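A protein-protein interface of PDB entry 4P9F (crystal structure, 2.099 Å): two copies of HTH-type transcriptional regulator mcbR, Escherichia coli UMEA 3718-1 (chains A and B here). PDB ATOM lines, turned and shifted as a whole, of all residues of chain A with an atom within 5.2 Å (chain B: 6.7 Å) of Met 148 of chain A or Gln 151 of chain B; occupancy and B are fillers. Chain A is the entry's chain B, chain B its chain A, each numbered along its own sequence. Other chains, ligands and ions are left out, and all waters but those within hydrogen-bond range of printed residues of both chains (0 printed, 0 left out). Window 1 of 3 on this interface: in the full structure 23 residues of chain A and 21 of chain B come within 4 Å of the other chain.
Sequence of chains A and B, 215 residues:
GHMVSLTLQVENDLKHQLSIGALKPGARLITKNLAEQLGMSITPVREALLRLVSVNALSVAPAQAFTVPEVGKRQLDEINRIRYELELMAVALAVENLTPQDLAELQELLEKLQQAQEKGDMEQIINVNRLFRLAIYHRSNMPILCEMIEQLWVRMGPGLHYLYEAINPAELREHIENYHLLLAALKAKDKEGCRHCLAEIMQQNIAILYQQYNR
Hydrophobic or aromatic side chains of chain A that line the printed part of chain B: Leu 86, Ile 144, Leu 145, Met 148 and Leu 152. Of the 19 printed residues of chain B, 6 touch a printed residue of chain A. Among the printed residues, 11 pairs touch across the chains. Among the printed residues, Asp or Glu carboxylates within 4 Å of a Lys or Arg side-chain nitrogen of the other chain: Glu 147 of chain A with Arg 155 of chain B (2.9 Å).
Met 148 of chain B touches Leu 86 of chain A (SD to CD1, 3.8 Å). Ile 144 of chain A touches Ile 79 of chain B. Ile 144 of chain A touches Ile 82 of chain B (CG2 to CD1, 3.9 Å). Ile 144 of chain A touches Arg 155 of chain B. Leu 145 of chain A touches Ile 82 of chain B. Val 55 of chain B touches Glu 147 of chain A. SD of Met 148 of chain A touches CG of Met 148 of chain B, at 3.9 Å. Gln 151 of chain B touches Met 148 of chain A. Met 148 of chain B touches Leu 152 of chain A.
Of chain B, only Met 148 (3.9 Å) and Gln 151 (3.4 Å) come within 4 Å of Met 148 of chain A. Gln 151 of chain B touches two residues of chain A. Printed residues of chain B within 4 Å of Ile 144 of chain A: Ile 79 (3.8 Å), Ile 82 (3.9 Å) and Arg 155 (3.6 Å). Of the printed residues of chain A, Ile 79 of chain B touches Ile 144 (3.8 Å). The nearest residue of chain B that does not touch Met 148 of chain A is Arg 155 of chain B (4.1 Å). The nearest printed residue of chain A that does not touch Arg 155 of chain B is Met 148 of chain A (4.1 Å).
The side-chain carboxylate of Glu 147 of chain B sits at hydrogen-bond distance from the side-chain amide nitrogen of Gln 151 of chain B, at 3.1 Å. The backbone carbonyl oxygen (O) of Val 55 of chain B lies within hydrogen-bond range of the guanidinium group (NH1) of Arg 155 of chain B.
Leu 86 of chain A touches Met 148 of chain B, but with the chains exchanged Met 148 of chain A does not touch Leu 86 of chain B (5.9 Å). Met 148 of chain A touches Gln 151 of chain B, but with the chains exchanged Gln 151 of chain A does not touch Met 148 of chain B (4.4 Å). Gln 151 of chain A touches its own counterpart, Gln 151 of chain B. Leu 152 of chain A touches Met 148 of chain B, but with the chains exchanged Met 148 of chain A does not touch Leu 152 of chain B (4.3 Å). Positions printed for both chains: 86, 144, 146, 147, 148, 149, 150, 151 and 152.
OE1 of Gln 151 of chain B sits at hydrogen-bond distance from NE2 of Gln 151 of chain A, at 2.5 Å. The guanidinium group of Arg 155 of chain B lies within salt-bridge range of the side-chain carboxylate of Glu 147 of chain A, 2.9 Å away.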
ATOM      1  N   LEU A  86      10.346 -20.890 -24.929  1.00  0.00           N
ATOM      2  CA  LEU A  86       9.653 -19.859 -24.148  1.00  0.00           C
ATOM      3  C   LEU A  86       8.153 -20.140 -23.987  1.00  0.00           C
ATOM      4  O   LEU A  86       7.586 -19.942 -22.910  1.00  0.00           O
ATOM      5  CB  LEU A  86       9.887 -18.484 -24.775  1.00  0.00           C
ATOM      6  CG  LEU A  86      11.372 -18.096 -24.732  1.00  0.00           C
ATOM      7  CD1 LEU A  86      11.600 -16.692 -25.239  1.00  0.00           C
ATOM      8  CD2 LEU A  86      11.919 -18.199 -23.309  1.00  0.00           C
ATOM      9  N   PRO A 143       5.154 -11.542 -16.930  1.00  0.00           N
ATOM     10  CA  PRO A 143       4.870 -10.557 -17.983  1.00  0.00           C
ATOM     11  C   PRO A 143       6.055 -10.365 -18.944  1.00  0.00           C
ATOM     12  O   PRO A 143       5.856 -10.122 -20.141  1.00  0.00           O
ATOM     13  CB  PRO A 143       4.560  -9.277 -17.193  1.00  0.00           C
ATOM     14  CG  PRO A 143       5.231  -9.463 -15.892  1.00  0.00           C
ATOM     15  CD  PRO A 143       5.179 -10.932 -15.590  1.00  0.00           C
ATOM     16  N   ILE A 144       7.272 -10.468 -18.422  1.00  0.00           N
ATOM     17  CA  ILE A 144       8.464 -10.287 -19.258  1.00  0.00           C
ATOM     18  C   ILE A 144       8.638 -11.462 -20.228  1.00  0.00           C
ATOM     19  O   ILE A 144       9.017 -11.261 -21.379  1.00  0.00           O
ATOM     20  CB  ILE A 144       9.743 -10.116 -18.405  1.00  0.00           C
ATOM     21  CG1 ILE A 144       9.577  -8.896 -17.475  1.00  0.00           C
ATOM     22  CG2 ILE A 144      10.965  -9.928 -19.327  1.00  0.00           C
ATOM     23  CD1 ILE A 144      10.750  -8.645 -16.543  1.00  0.00           C
ATOM     24  N   LEU A 145       8.343 -12.675 -19.762  1.00  0.00           N
ATOM     25  CA  LEU A 145       8.339 -13.852 -20.614  1.00  0.00           C
ATOM     26  C   LEU A 145       7.334 -13.659 -21.752  1.00  0.00           C
ATOM     27  O   LEU A 145       7.641 -13.921 -22.907  1.00  0.00           O
ATOM     28  CB  LEU A 145       8.000 -15.113 -19.792  1.00  0.00           C
ATOM     29  CG  LEU A 145       7.741 -16.434 -20.516  1.00  0.00           C
ATOM     30  CD1 LEU A 145       8.913 -16.863 -21.391  1.00  0.00           C
ATOM     31  CD2 LEU A 145       7.435 -17.523 -19.473  1.00  0.00           C
ATOM     32  N   CYS A 146       6.134 -13.194 -21.417  1.00  0.00           N
ATOM     33  CA  CYS A 146       5.106 -12.923 -22.429  1.00  0.00           C
ATOM     34  C   CYS A 146       5.548 -11.846 -23.422  1.00  0.00           C
ATOM     35  O   CYS A 146       5.269 -11.969 -24.622  1.00  0.00           O
ATOM     36  CB  CYS A 146       3.778 -12.540 -21.759  1.00  0.00           C
ATOM     37  SG  CYS A 146       3.107 -13.921 -20.775  1.00  0.00           S
ATOM     38  N   GLU A 147       6.232 -10.805 -22.940  1.00  0.00           N
ATOM     39  CA  GLU A 147       6.780  -9.786 -23.831  1.00  0.00           C
ATOM     40  C   GLU A 147       7.694 -10.457 -24.859  1.00  0.00           C
ATOM     41  O   GLU A 147       7.613 -10.194 -26.059  1.00  0.00           O
ATOM     42  CB  GLU A 147       7.616  -8.742 -23.072  1.00  0.00           C
ATOM     43  CG  GLU A 147       6.881  -7.725 -22.220  1.00  0.00           C
ATOM     44  CD  GLU A 147       7.868  -6.781 -21.540  1.00  0.00           C
ATOM     45  OE1 GLU A 147       8.820  -6.308 -22.219  1.00  0.00           O
ATOM     46  OE2 GLU A 147       7.711  -6.537 -20.329  1.00  0.00           O
ATOM     47  N   MET A 148       8.581 -11.321 -24.371  1.00  0.00           N
ATOM     48  CA  MET A 148       9.536 -11.975 -25.260  1.00  0.00           C
ATOM     49  C   MET A 148       8.809 -12.814 -26.317  1.00  0.00           C
ATOM     50  O   MET A 148       9.182 -12.801 -27.487  1.00  0.00           O
ATOM     51  CB  MET A 148      10.517 -12.851 -24.467  1.00  0.00           C
ATOM     52  CG  MET A 148      11.420 -12.096 -23.448  1.00  0.00           C
ATOM     53  SD  MET A 148      12.444 -10.625 -24.284  1.00  0.00           S
ATOM     54  CE  MET A 148      11.374  -9.129 -23.632  1.00  0.00           C
ATOM     55  N   ILE A 149       7.793 -13.565 -25.896  1.00  0.00           N
ATOM     56  CA  ILE A 149       7.013 -14.377 -26.827  1.00  0.00           C
ATOM     57  C   ILE A 149       6.295 -13.515 -27.885  1.00  0.00           C
ATOM     58  O   ILE A 149       6.309 -13.837 -29.082  1.00  0.00           O
ATOM     59  CB  ILE A 149       5.979 -15.251 -26.071  1.00  0.00           C
ATOM     60  CG1 ILE A 149       6.708 -16.276 -25.190  1.00  0.00           C
ATOM     61  CG2 ILE A 149       5.032 -15.935 -27.076  1.00  0.00           C
ATOM     62  CD1 ILE A 149       5.842 -17.027 -24.227  1.00  0.00           C
ATOM     63  N   GLU A 150       5.670 -12.420 -27.463  1.00  0.00           N
ATOM     64  CA  GLU A 150       5.046 -11.513 -28.433  1.00  0.00           C
ATOM     65  C   GLU A 150       6.045 -10.904 -29.412  1.00  0.00           C
ATOM     66  O   GLU A 150       5.721 -10.677 -30.583  1.00  0.00           O
ATOM     67  CB  GLU A 150       4.286 -10.390 -27.718  1.00  0.00           C
ATOM     68  CG  GLU A 150       3.034 -10.904 -27.041  1.00  0.00           C
ATOM     69  CD  GLU A 150       2.036  -9.797 -26.744  1.00  0.00           C
ATOM     70  OE1 GLU A 150       2.052  -9.261 -25.625  1.00  0.00           O
ATOM     71  OE2 GLU A 150       1.232  -9.482 -27.645  1.00  0.00           O
ATOM     72  N   GLN A 151       7.256 -10.621 -28.940  1.00  0.00           N
ATOM     73  CA  GLN A 151       8.296 -10.087 -29.843  1.00  0.00           C
ATOM     74  C   GLN A 151       8.587 -11.049 -30.978  1.00  0.00           C
ATOM     75  O   GLN A 151       8.728 -10.665 -32.136  1.00  0.00           O
ATOM     76  CB  GLN A 151       9.593  -9.823 -29.082  1.00  0.00           C
ATOM     77  CG  GLN A 151       9.624  -8.515 -28.362  1.00  0.00           C
ATOM     78  CD  GLN A 151      11.014  -8.164 -27.860  1.00  0.00           C
ATOM     79  OE1 GLN A 151      12.028  -8.608 -28.399  1.00  0.00           O
ATOM     80  NE2 GLN A 151      11.057  -7.354 -26.830  1.00  0.00           N
ATOM     81  N   LEU A 152       8.680 -12.316 -30.619  1.00  0.00           N
ATOM     82  CA  LEU A 152       8.982 -13.364 -31.582  1.00  0.00           C
ATOM     83  C   LEU A 152       7.824 -13.562 -32.540  1.00  0.00           C
ATOM     84  O   LEU A 152       8.030 -13.893 -33.707  1.00  0.00           O
ATOM     85  CB  LEU A 152       9.301 -14.661 -30.857  1.00  0.00           C
ATOM     86  CG  LEU A 152      10.641 -14.604 -30.099  1.00  0.00           C
ATOM     87  CD1 LEU A 152      10.728 -15.740 -29.143  1.00  0.00           C
ATOM     88  CD2 LEU A 152      11.807 -14.679 -31.075  1.00  0.00           C
ATOM     89  N   LYS B  15      22.129   1.304 -23.823  1.00  0.00           N
ATOM     90  CA  LYS B  15      21.985  -0.137 -23.538  1.00  0.00           C
ATOM     91  C   LYS B  15      23.187  -0.642 -22.748  1.00  0.00           C
ATOM     92  O   LYS B  15      23.046  -1.393 -21.777  1.00  0.00           O
ATOM     93  CB  LYS B  15      21.833  -0.930 -24.827  1.00  0.00           C
ATOM     94  CG  LYS B  15      20.460  -0.796 -25.506  1.00  0.00           C
ATOM     95  CD  LYS B  15      20.408  -1.660 -26.796  1.00  0.00           C
ATOM     96  CE  LYS B  15      19.013  -1.638 -27.454  1.00  0.00           C
ATOM     97  NZ  LYS B  15      18.931  -2.478 -28.720  1.00  0.00           N
ATOM     98  N   SER B  19      23.132  -2.067 -19.027  1.00  0.00           N
ATOM     99  CA  SER B  19      23.604  -3.443 -18.881  1.00  0.00           C
ATOM    100  C   SER B  19      24.702  -3.646 -17.834  1.00  0.00           C
ATOM    101  O   SER B  19      24.725  -4.682 -17.150  1.00  0.00           O
ATOM    102  CB  SER B  19      24.143  -3.960 -20.216  1.00  0.00           C
ATOM    103  OG  SER B  19      23.103  -4.024 -21.168  1.00  0.00           O
ATOM    104  N   VAL B  55      10.760  -1.082 -25.698  1.00  0.00           N
ATOM    105  CA  VAL B  55      11.025  -2.448 -25.236  1.00  0.00           C
ATOM    106  C   VAL B  55      11.006  -2.537 -23.699  1.00  0.00           C
ATOM    107  O   VAL B  55      11.466  -3.528 -23.122  1.00  0.00           O
ATOM    108  CB  VAL B  55      12.367  -3.009 -25.800  1.00  0.00           C
ATOM    109  CG1 VAL B  55      12.299  -3.075 -27.317  1.00  0.00           C
ATOM    110  CG2 VAL B  55      13.573  -2.192 -25.312  1.00  0.00           C
ATOM    111  N   ALA B  57      12.723  -1.014 -21.459  1.00  0.00           N
ATOM    112  CA  ALA B  57      14.036  -0.865 -20.840  1.00  0.00           C
ATOM    113  C   ALA B  57      14.139   0.450 -20.077  1.00  0.00           C
ATOM    114  O   ALA B  57      15.042   0.639 -19.254  1.00  0.00           O
ATOM    115  CB  ALA B  57      15.129  -0.951 -21.892  1.00  0.00           C
ATOM    116  N   ILE B  79      13.593 -12.491 -14.986  1.00  0.00           N
ATOM    117  CA  ILE B  79      14.624 -12.262 -15.999  1.00  0.00           C
ATOM    118  C   ILE B  79      15.682 -13.365 -15.961  1.00  0.00           C
ATOM    119  O   ILE B  79      16.124 -13.850 -17.008  1.00  0.00           O
ATOM    120  CB  ILE B  79      15.309 -10.893 -15.797  1.00  0.00           C
ATOM    121  CG1 ILE B  79      14.305  -9.771 -16.079  1.00  0.00           C
ATOM    122  CG2 ILE B  79      16.558 -10.764 -16.692  1.00  0.00           C
ATOM    123  CD1 ILE B  79      14.778  -8.381 -15.651  1.00  0.00           C
ATOM    124  N   ILE B  82      14.277 -16.671 -17.398  1.00  0.00           N
ATOM    125  CA  ILE B  82      14.214 -16.613 -18.850  1.00  0.00           C
ATOM    126  C   ILE B  82      15.608 -16.745 -19.460  1.00  0.00           C
ATOM    127  O   ILE B  82      15.838 -17.568 -20.343  1.00  0.00           O
ATOM    128  CB  ILE B  82      13.567 -15.300 -19.354  1.00  0.00           C
ATOM    129  CG1 ILE B  82      12.140 -15.144 -18.806  1.00  0.00           C
ATOM    130  CG2 ILE B  82      13.537 -15.285 -20.892  1.00  0.00           C
ATOM    131  CD1 ILE B  82      11.541 -13.749 -19.015  1.00  0.00           C
ATOM    132  N   LEU B  86      17.852 -19.369 -22.243  1.00  0.00           N
ATOM    133  CA  LEU B  86      18.372 -18.832 -23.498  1.00  0.00           C
ATOM    134  C   LEU B  86      19.888 -18.907 -23.577  1.00  0.00           C
ATOM    135  O   LEU B  86      20.440 -19.249 -24.626  1.00  0.00           O
ATOM    136  CB  LEU B  86      17.923 -17.384 -23.680  1.00  0.00           C
ATOM    137  CG  LEU B  86      16.399 -17.200 -23.767  1.00  0.00           C
ATOM    138  CD1 LEU B  86      15.992 -15.742 -24.075  1.00  0.00           C
ATOM    139  CD2 LEU B  86      15.770 -18.180 -24.778  1.00  0.00           C
ATOM    140  N   ILE B 144      19.066 -13.581 -33.409  1.00  0.00           N
ATOM    141  CA  ILE B 144      17.868 -13.210 -32.659  1.00  0.00           C
ATOM    142  C   ILE B 144      17.950 -13.719 -31.216  1.00  0.00           C
ATOM    143  O   ILE B 144      17.551 -13.021 -30.264  1.00  0.00           O
ATOM    144  CB  ILE B 144      16.596 -13.749 -33.342  1.00  0.00           C
ATOM    145  CG1 ILE B 144      16.499 -13.184 -34.769  1.00  0.00           C
ATOM    146  CG2 ILE B 144      15.359 -13.348 -32.560  1.00  0.00           C
ATOM    147  CD1 ILE B 144      15.252 -13.639 -35.528  1.00  0.00           C
ATOM    148  N   CYS B 146      20.800 -14.225 -29.584  1.00  0.00           N
ATOM    149  CA  CYS B 146      21.779 -13.343 -28.943  1.00  0.00           C
ATOM    150  C   CYS B 146      21.232 -11.956 -28.599  1.00  0.00           C
ATOM    151  O   CYS B 146      21.482 -11.456 -27.506  1.00  0.00           O
ATOM    152  CB  CYS B 146      23.009 -13.185 -29.853  1.00  0.00           C
ATOM    153  SG  CYS B 146      23.923 -14.764 -30.059  1.00  0.00           S
ATOM    154  N   GLU B 147      20.489 -11.345 -29.523  1.00  0.00           N
ATOM    155  CA  GLU B 147      19.878 -10.036 -29.269  1.00  0.00           C
ATOM    156  C   GLU B 147      18.925 -10.118 -28.090  1.00  0.00           C
ATOM    157  O   GLU B 147      18.867  -9.221 -27.258  1.00  0.00           O
ATOM    158  CB  GLU B 147      19.136  -9.496 -30.506  1.00  0.00           C
ATOM    159  CG  GLU B 147      18.859  -7.951 -30.466  1.00  0.00           C
ATOM    160  CD  GLU B 147      17.648  -7.511 -29.597  1.00  0.00           C
ATOM    161  OE1 GLU B 147      16.718  -8.320 -29.364  1.00  0.00           O
ATOM    162  OE2 GLU B 147      17.619  -6.333 -29.154  1.00  0.00           O
ATOM    163  N   MET B 148      18.161 -11.198 -28.018  1.00  0.00           N
ATOM    164  CA  MET B 148      17.221 -11.351 -26.910  1.00  0.00           C
ATOM    165  C   MET B 148      17.965 -11.467 -25.573  1.00  0.00           C
ATOM    166  O   MET B 148      17.538 -10.915 -24.552  1.00  0.00           O
ATOM    167  CB  MET B 148      16.325 -12.575 -27.117  1.00  0.00           C
ATOM    168  CG  MET B 148      15.291 -12.716 -26.003  1.00  0.00           C
ATOM    169  SD  MET B 148      13.778 -13.844 -26.481  1.00  0.00           S
ATOM    170  CE  MET B 148      13.186 -12.811 -28.018  1.00  0.00           C
ATOM    171  N   ILE B 149      19.080 -12.182 -25.586  1.00  0.00           N
ATOM    172  CA  ILE B 149      19.914 -12.300 -24.390  1.00  0.00           C
ATOM    173  C   ILE B 149      20.426 -10.902 -23.989  1.00  0.00           C
ATOM    174  O   ILE B 149      20.339 -10.517 -22.828  1.00  0.00           O
ATOM    175  CB  ILE B 149      21.089 -13.292 -24.612  1.00  0.00           C
ATOM    176  CG1 ILE B 149      20.552 -14.734 -24.744  1.00  0.00           C
ATOM    177  CG2 ILE B 149      22.121 -13.201 -23.460  1.00  0.00           C
ATOM    178  CD1 ILE B 149      21.629 -15.773 -25.160  1.00  0.00           C
ATOM    179  N   GLU B 150      20.898 -10.126 -24.957  1.00  0.00           N
ATOM    180  CA  GLU B 150      21.341  -8.754 -24.668  1.00  0.00           C
ATOM    181  C   GLU B 150      20.205  -7.905 -24.117  1.00  0.00           C
ATOM    182  O   GLU B 150      20.395  -7.091 -23.201  1.00  0.00           O
ATOM    183  CB  GLU B 150      21.887  -8.104 -25.936  1.00  0.00           C
ATOM    184  CG  GLU B 150      23.196  -8.683 -26.397  1.00  0.00           C
ATOM    185  CD  GLU B 150      23.855  -7.815 -27.438  1.00  0.00           C
ATOM    186  OE1 GLU B 150      23.567  -8.044 -28.623  1.00  0.00           O
ATOM    187  OE2 GLU B 150      24.622  -6.893 -27.082  1.00  0.00           O
ATOM    188  N   GLN B 151      19.012  -8.109 -24.666  1.00  0.00           N
ATOM    189  CA  GLN B 151      17.825  -7.382 -24.213  1.00  0.00           C
ATOM    190  C   GLN B 151      17.556  -7.663 -22.719  1.00  0.00           C
ATOM    191  O   GLN B 151      17.277  -6.759 -21.928  1.00  0.00           O
ATOM    192  CB  GLN B 151      16.636  -7.798 -25.066  1.00  0.00           C
ATOM    193  CG  GLN B 151      15.600  -6.751 -25.295  1.00  0.00           C
ATOM    194  CD  GLN B 151      14.395  -7.300 -26.037  1.00  0.00           C
ATOM    195  OE1 GLN B 151      13.267  -7.128 -25.604  1.00  0.00           O
ATOM    196  NE2 GLN B 151      14.638  -7.973 -27.153  1.00  0.00           N
ATOM    197  N   LEU B 152      17.672  -8.927 -22.332  1.00  0.00           N
ATOM    198  CA  LEU B 152      17.417  -9.309 -20.942  1.00  0.00           C
ATOM    199  C   LEU B 152      18.505  -8.764 -20.003  1.00  0.00           C
ATOM    200  O   LEU B 152      18.222  -8.396 -18.867  1.00  0.00           O
ATOM    201  CB  LEU B 152      17.290 -10.826 -20.844  1.00  0.00           C
ATOM    202  CG  LEU B 152      16.007 -11.364 -21.509  1.00  0.00           C
ATOM    203  CD1 LEU B 152      16.061 -12.891 -21.718  1.00  0.00           C
ATOM    204  CD2 LEU B 152      14.766 -10.995 -20.666  1.00  0.00           C
ATOM    205  N   TRP B 153      19.740  -8.672 -20.489  1.00  0.00           N
ATOM    206  CA  TRP B 153      20.811  -8.054 -19.710  1.00  0.00           C
ATOM    207  C   TRP B 153      20.538  -6.574 -19.454  1.00  0.00           C
ATOM    208  O   TRP B 153      20.891  -6.035 -18.401  1.00  0.00           O
ATOM    209  CB  TRP B 153      22.140  -8.200 -20.442  1.00  0.00           C
ATOM    210  CG  TRP B 153      22.718  -9.589 -20.406  1.00  0.00           C
ATOM    211  CD1 TRP B 153      22.289 -10.649 -19.654  1.00  0.00           C
ATOM    212  CD2 TRP B 153      23.795 -10.080 -21.220  1.00  0.00           C
ATOM    213  NE1 TRP B 153      23.064 -11.762 -19.922  1.00  0.00           N
ATOM    214  CE2 TRP B 153      23.993 -11.438 -20.883  1.00  0.00           C
ATOM    215  CE3 TRP B 153      24.623  -9.495 -22.204  1.00  0.00           C
ATOM    216  CZ2 TRP B 153      24.983 -12.223 -21.485  1.00  0.00           C
ATOM    217  CZ3 TRP B 153      25.608 -10.278 -22.803  1.00  0.00           C
ATOM    218  CH2 TRP B 153      25.784 -11.625 -22.435  1.00  0.00           C
ATOM    219  N   VAL B 154      19.963  -5.909 -20.454  1.00  0.00           N
ATOM    220  CA  VAL B 154      19.559  -4.510 -20.317  1.00  0.00           C
ATOM    221  C   VAL B 154      18.474  -4.379 -19.247  1.00  0.00           C
ATOM    222  O   VAL B 154      18.522  -3.471 -18.433  1.00  0.00           O
ATOM    223  CB  VAL B 154      19.039  -3.924 -21.648  1.00  0.00           C
ATOM    224  CG1 VAL B 154      18.421  -2.533 -21.422  1.00  0.00           C
ATOM    225  CG2 VAL B 154      20.178  -3.830 -22.694  1.00  0.00           C
ATOM    226  N   ARG B 155      17.507  -5.294 -19.251  1.00  0.00           N
ATOM    227  CA  ARG B 155      16.398  -5.275 -18.288  1.00  0.00           C
ATOM    228  C   ARG B 155      16.902  -5.519 -16.849  1.00  0.00           C
ATOM    229  O   ARG B 155      16.473  -4.861 -15.918  1.00  0.00           O
ATOM    230  CB  ARG B 155      15.351  -6.342 -18.670  1.00  0.00           C
ATOM    231  CG  ARG B 155      14.607  -6.053 -19.964  1.00  0.00           C
ATOM    232  CD  ARG B 155      13.728  -4.827 -19.873  1.00  0.00           C
ATOM    233  NE  ARG B 155      12.479  -5.013 -19.121  1.00  0.00           N
ATOM    234  CZ  ARG B 155      11.382  -5.557 -19.661  1.00  0.00           C
ATOM    235  NH1 ARG B 155      11.417  -6.011 -20.907  1.00  0.00           N
ATOM    236  NH2 ARG B 155      10.263  -5.659 -18.968  1.00  0.00           N
ATOM    237  N   MET B 156      17.809  -6.475 -16.663  1.00  0.00           N
ATOM    238  CA  MET B 156      18.303  -6.722 -15.312  1.00  0.00           C
ATOM    239  C   MET B 156      19.379  -5.726 -14.901  1.00  0.00           C
ATOM    240  O   MET B 156      19.667  -5.590 -13.709  1.00  0.00           O
ATOM    241  CB  MET B 156      18.839  -8.140 -15.170  1.00  0.00           C
ATOM    242  CG  MET B 156      20.102  -8.429 -15.919  1.00  0.00           C
ATOM    243  SD  MET B 156      20.630 -10.305 -15.621  1.00  0.00           S
ATOM    244  CE  MET B 156      21.143 -10.209 -13.839  1.00  0.00           C
